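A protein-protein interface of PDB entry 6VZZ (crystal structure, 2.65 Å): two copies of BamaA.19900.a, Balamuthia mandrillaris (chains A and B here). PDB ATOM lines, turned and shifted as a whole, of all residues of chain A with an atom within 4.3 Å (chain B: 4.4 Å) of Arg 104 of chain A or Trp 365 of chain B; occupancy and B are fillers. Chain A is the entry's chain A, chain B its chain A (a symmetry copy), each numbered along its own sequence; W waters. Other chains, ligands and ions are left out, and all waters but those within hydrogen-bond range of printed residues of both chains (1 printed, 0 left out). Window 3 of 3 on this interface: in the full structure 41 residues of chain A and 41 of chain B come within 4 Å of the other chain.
No position is printed for both chains. Of the 7 pairs that touch across the chains among the printed residues, none has its exchanged pair printed and touching as well.
Of the 9 printed residues of chain A, 4 touch a printed residue of chain B. Printed residues of chain A that touch a printed residue of chain B: Arg 104, Thr 115, Glu 218 and His 221. Hydrophobic or aromatic side chains of chain A within 4 Å of the printed part of chain B: His 221. Hydrophobic or aromatic side chains of chain B that line the printed part of chain A: Trp 365. Among the printed residues, 7 pairs touch across the chains. Among the printed residues, no Asp or Glu carboxylate lies within 4 Å of a Lys or Arg side-chain nitrogen of the other chain.
The side-chain amino group (NZ) of Lys 362 of chain B is in hydrogen-bond range of a ring nitrogen (ND1) of His 221 of chain A, at 3.5 Å. The indole nitrogen (NE1) of Trp 365 of chain B lies close to the guanidinium group (NH1) of Arg 104 of chain A.
OD2 of Asp 113 of chain A is in salt-bridge range of NH1 of Arg 104 of chain A, at 3.8 Å. NE2 of His 221 of chain A lies close to OE1 of Glu 218 of chain A (3.3 Å).
Among the printed residues, pairs that only touch across the chains: Arg 104 of chain A with Gln 328 of chain B, His 221 of chain A with Trp 365 of chain B, Glu 218 of chain A with Gln 328 of chain B, Glu 218 of chain A with Trp 365 of chain B and Thr 115 of chain A with Trp 365 of chain B.
Arg 104 of chain A touches two residues of chain B. Ile 105 of chain A touches none of the printed residues of chain B. Leu 112 of chain A touches none of the printed residues of chain B. Printed residues of chain B within 4 Å of Thr 115 of chain A: Trp 365. Of the printed residues of chain B, Glu 218 of chain A touches Gln 328 (3.8 Å) and Trp 365 (3.9 Å). Of the printed residues of chain B, His 221 of chain A touches Lys 362 (3.5 Å) and Trp 365 (3.8 Å). Printed residues of chain A within 4 Å of Gln 328 of chain B: Arg 104 and Glu 218. Printed residues of chain A within 4 Å of Lys 362 of chain B: His 221 (3.5 Å). Trp 365 of chain B touches four residues of chain A. The nearest printed residue of chain A that does not touch Trp 365 of chain B is Asp 113 of chain A (6.0 Å).
Water W1 lies within hydrogen-bond range of the side-chain amide oxygen of Gln 328 of chain B (2.8 Å) and the guanidinium group of Arg 104 of chain A (2.8 Å).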
ATOM      1  N   GLY A 103       3.400  15.977 -22.851  1.00  0.00           N
ATOM      2  CA  GLY A 103       4.738  16.433 -22.555  1.00  0.00           C
ATOM      3  C   GLY A 103       5.677  15.273 -22.340  1.00  0.00           C
ATOM      4  O   GLY A 103       5.399  14.145 -22.751  1.00  0.00           O
ATOM      5  N   ARG A 104       6.791  15.563 -21.677  1.00  0.00           N
ATOM      6  CA  ARG A 104       7.880  14.620 -21.484  1.00  0.00           C
ATOM      7  C   ARG A 104       7.773  13.965 -20.123  1.00  0.00           C
ATOM      8  O   ARG A 104       7.197  14.519 -19.187  1.00  0.00           O
ATOM      9  CB  ARG A 104       9.231  15.319 -21.608  1.00  0.00           C
ATOM     10  CG  ARG A 104       9.551  15.811 -22.993  1.00  0.00           C
ATOM     11  CD  ARG A 104      10.120  17.197 -22.941  1.00  0.00           C
ATOM     12  NE  ARG A 104      11.405  17.241 -22.251  1.00  0.00           N
ATOM     13  CZ  ARG A 104      11.648  17.983 -21.171  1.00  0.00           C
ATOM     14  NH1 ARG A 104      10.694  18.755 -20.642  1.00  0.00           N
ATOM     15  NH2 ARG A 104      12.854  17.954 -20.623  1.00  0.00           N
ATOM     16  N   ILE A 105       8.367  12.784 -20.013  1.00  0.00           N
ATOM     17  CA  ILE A 105       8.320  11.993 -18.792  1.00  0.00           C
ATOM     18  C   ILE A 105       9.738  11.662 -18.355  1.00  0.00           C
ATOM     19  O   ILE A 105      10.570  11.261 -19.177  1.00  0.00           O
ATOM     20  CB  ILE A 105       7.496  10.715 -18.997  1.00  0.00           C
ATOM     21  CG1 ILE A 105       6.080  11.119 -19.358  1.00  0.00           C
ATOM     22  CG2 ILE A 105       7.532   9.827 -17.756  1.00  0.00           C
ATOM     23  CD1 ILE A 105       5.402  10.094 -20.117  1.00  0.00           C
ATOM     24  N   VAL A 111       7.535  11.609 -13.052  1.00  0.00           N
ATOM     25  CA  VAL A 111       7.173  13.011 -13.243  1.00  0.00           C
ATOM     26  C   VAL A 111       6.766  13.252 -14.694  1.00  0.00           C
ATOM     27  O   VAL A 111       7.471  12.834 -15.620  1.00  0.00           O
ATOM     28  CB  VAL A 111       8.337  13.954 -12.868  1.00  0.00           C
ATOM     29  CG1 VAL A 111       7.901  15.412 -12.969  1.00  0.00           C
ATOM     30  CG2 VAL A 111       8.881  13.624 -11.488  1.00  0.00           C
ATOM     31  N   LEU A 112       5.649  13.953 -14.885  1.00  0.00           N
ATOM     32  CA  LEU A 112       5.223  14.461 -16.182  1.00  0.00           C
ATOM     33  C   LEU A 112       5.448  15.968 -16.226  1.00  0.00           C
ATOM     34  O   LEU A 112       5.191  16.671 -15.245  1.00  0.00           O
ATOM     35  CB  LEU A 112       3.744  14.137 -16.440  1.00  0.00           C
ATOM     36  CG  LEU A 112       3.016  14.881 -17.566  1.00  0.00           C
ATOM     37  CD1 LEU A 112       3.482  14.444 -18.957  1.00  0.00           C
ATOM     38  CD2 LEU A 112       1.523  14.709 -17.428  1.00  0.00           C
ATOM     39  N   ASP A 113       5.942  16.460 -17.361  1.00  0.00           N
ATOM     40  CA  ASP A 113       6.200  17.881 -17.596  1.00  0.00           C
ATOM     41  C   ASP A 113       5.309  18.279 -18.773  1.00  0.00           C
ATOM     42  O   ASP A 113       5.595  17.916 -19.920  1.00  0.00           O
ATOM     43  CB  ASP A 113       7.690  18.113 -17.885  1.00  0.00           C
ATOM     44  CG  ASP A 113       8.079  19.591 -17.939  1.00  0.00           C
ATOM     45  OD1 ASP A 113       7.369  20.410 -18.566  1.00  0.00           O
ATOM     46  OD2 ASP A 113       9.127  19.936 -17.350  1.00  0.00           O
ATOM     47  N   THR A 115       4.167  20.354 -21.573  1.00  0.00           N
ATOM     48  CA  THR A 115       4.974  21.344 -22.278  1.00  0.00           C
ATOM     49  C   THR A 115       4.295  22.709 -22.328  1.00  0.00           C
ATOM     50  O   THR A 115       4.957  23.743 -22.185  1.00  0.00           O
ATOM     51  CB  THR A 115       5.278  20.843 -23.688  1.00  0.00           C
ATOM     52  OG1 THR A 115       5.994  19.607 -23.601  1.00  0.00           O
ATOM     53  CG2 THR A 115       6.103  21.866 -24.471  1.00  0.00           C
ATOM     54  N   GLU A 218       9.260  14.221 -30.006  1.00  0.00           N
ATOM     55  CA  GLU A 218       8.981  15.627 -29.746  1.00  0.00           C
ATOM     56  C   GLU A 218       9.228  16.483 -30.983  1.00  0.00           C
ATOM     57  O   GLU A 218       9.643  17.637 -30.876  1.00  0.00           O
ATOM     58  CB  GLU A 218       9.814  16.126 -28.570  1.00  0.00           C
ATOM     59  CG  GLU A 218       9.337  15.608 -27.226  1.00  0.00           C
ATOM     60  CD  GLU A 218       7.963  16.150 -26.866  1.00  0.00           C
ATOM     61  OE1 GLU A 218       7.590  17.245 -27.373  1.00  0.00           O
ATOM     62  OE2 GLU A 218       7.248  15.471 -26.093  1.00  0.00           O
ATOM     63  N   HIS A 221       8.623  20.385 -32.023  1.00  0.00           N
ATOM     64  CA  HIS A 221       9.429  21.493 -31.546  1.00  0.00           C
ATOM     65  C   HIS A 221      10.707  21.703 -32.351  1.00  0.00           C
ATOM     66  O   HIS A 221      11.509  22.566 -31.990  1.00  0.00           O
ATOM     67  CB  HIS A 221       9.739  21.288 -30.062  1.00  0.00           C
ATOM     68  CG  HIS A 221       8.509  21.122 -29.225  1.00  0.00           C
ATOM     69  ND1 HIS A 221       7.671  22.175 -28.918  1.00  0.00           N
ATOM     70  CD2 HIS A 221       7.958  20.024 -28.654  1.00  0.00           C
ATOM     71  CE1 HIS A 221       6.663  21.733 -28.185  1.00  0.00           C
ATOM     72  NE2 HIS A 221       6.816  20.433 -28.010  1.00  0.00           N
ATOM     73  N   GLN B 328      14.516  12.660 -28.640  1.00  0.00           N
ATOM     74  CA  GLN B 328      14.669  12.586 -27.188  1.00  0.00           C
ATOM     75  C   GLN B 328      15.781  11.617 -26.800  1.00  0.00           C
ATOM     76  O   GLN B 328      15.622  10.777 -25.912  1.00  0.00           O
ATOM     77  CB  GLN B 328      13.353  12.199 -26.512  1.00  0.00           C
ATOM     78  CG  GLN B 328      12.307  13.282 -26.507  1.00  0.00           C
ATOM     79  CD  GLN B 328      12.721  14.491 -25.676  1.00  0.00           C
ATOM     80  OE1 GLN B 328      12.732  14.435 -24.446  1.00  0.00           O
ATOM     81  NE2 GLN B 328      13.056  15.592 -26.345  1.00  0.00           N
ATOM     82  N   LYS B 362      13.932  25.444 -26.980  1.00  0.00           N
ATOM     83  CA  LYS B 362      13.953  24.360 -26.003  1.00  0.00           C
ATOM     84  C   LYS B 362      15.371  23.996 -25.602  1.00  0.00           C
ATOM     85  O   LYS B 362      15.671  22.822 -25.376  1.00  0.00           O
ATOM     86  CB  LYS B 362      13.232  23.136 -26.559  1.00  0.00           C
ATOM     87  CG  LYS B 362      11.794  23.377 -26.966  1.00  0.00           C
ATOM     88  CD  LYS B 362      10.938  23.763 -25.784  1.00  0.00           C
ATOM     89  CE  LYS B 362       9.451  23.581 -26.097  1.00  0.00           C
ATOM     90  NZ  LYS B 362       8.846  24.715 -26.847  1.00  0.00           N
ATOM     91  N   LYS B 363      16.273  24.975 -25.514  1.00  0.00           N
ATOM     92  CA  LYS B 363      17.667  24.641 -25.236  1.00  0.00           C
ATOM     93  C   LYS B 363      17.816  23.957 -23.885  1.00  0.00           C
ATOM     94  O   LYS B 363      18.702  23.114 -23.713  1.00  0.00           O
ATOM     95  CB  LYS B 363      18.543  25.892 -25.323  1.00  0.00           C
ATOM     96  CG  LYS B 363      18.666  26.692 -24.066  1.00  0.00           C
ATOM     97  CD  LYS B 363      19.414  27.988 -24.342  1.00  0.00           C
ATOM     98  CE  LYS B 363      18.540  28.983 -25.113  1.00  0.00           C
ATOM     99  NZ  LYS B 363      19.355  29.912 -25.961  1.00  0.00           N
ATOM    100  N   ALA B 364      16.931  24.268 -22.937  1.00  0.00           N
ATOM    101  CA  ALA B 364      16.954  23.590 -21.648  1.00  0.00           C
ATOM    102  C   ALA B 364      16.813  22.077 -21.797  1.00  0.00           C
ATOM    103  O   ALA B 364      17.356  21.323 -20.980  1.00  0.00           O
ATOM    104  CB  ALA B 364      15.850  24.148 -20.748  1.00  0.00           C
ATOM    105  N   TRP B 365      16.112  21.613 -22.843  1.00  0.00           N
ATOM    106  CA  TRP B 365      15.897  20.177 -23.019  1.00  0.00           C
ATOM    107  C   TRP B 365      17.167  19.448 -23.435  1.00  0.00           C
ATOM    108  O   TRP B 365      17.304  18.254 -23.162  1.00  0.00           O
ATOM    109  CB  TRP B 365      14.815  19.904 -24.068  1.00  0.00           C
ATOM    110  CG  TRP B 365      13.439  20.330 -23.696  1.00  0.00           C
ATOM    111  CD1 TRP B 365      13.076  21.087 -22.625  1.00  0.00           C
ATOM    112  CD2 TRP B 365      12.229  20.022 -24.397  1.00  0.00           C
ATOM    113  NE1 TRP B 365      11.718  21.279 -22.616  1.00  0.00           N
ATOM    114  CE2 TRP B 365      11.170  20.636 -23.692  1.00  0.00           C
ATOM    115  CE3 TRP B 365      11.935  19.284 -25.549  1.00  0.00           C
ATOM    116  CZ2 TRP B 365       9.834  20.534 -24.097  1.00  0.00           C
ATOM    117  CZ3 TRP B 365      10.609  19.185 -25.957  1.00  0.00           C
ATOM    118  CH2 TRP B 365       9.573  19.807 -25.228  1.00  0.00           C
ATOM    119  N   ILE B 366      18.091  20.119 -24.115  1.00  0.00           N
ATOM    120  CA  ILE B 366      19.283  19.450 -24.615  1.00  0.00           C
ATOM    121  C   ILE B 366      20.535  19.845 -23.840  1.00  0.00           C
ATOM    122  O   ILE B 366      21.640  19.466 -24.234  1.00  0.00           O
ATOM    123  CB  ILE B 366      19.470  19.687 -26.120  1.00  0.00           C
ATOM    124  CG1 ILE B 366      19.401  21.186 -26.442  1.00  0.00           C
ATOM    125  CG2 ILE B 366      18.424  18.900 -26.901  1.00  0.00           C
ATOM    126  CD1 ILE B 366      19.632  21.517 -27.912  1.00  0.00           C
ATOM    127  N   GLU B 367      20.390  20.571 -22.729  1.00  0.00           N
ATOM    128  CA  GLU B 367      21.557  20.984 -21.952  1.00  0.00           C
ATOM    129  C   GLU B 367      22.377  19.789 -21.462  1.00  0.00           C
ATOM    130  O   GLU B 367      23.604  19.885 -21.357  1.00  0.00           O
ATOM    131  CB  GLU B 367      21.121  21.861 -20.775  1.00  0.00           C
HETATM  132  O   HOH W   1      13.967  16.299 -22.832  1.00  0.00           O
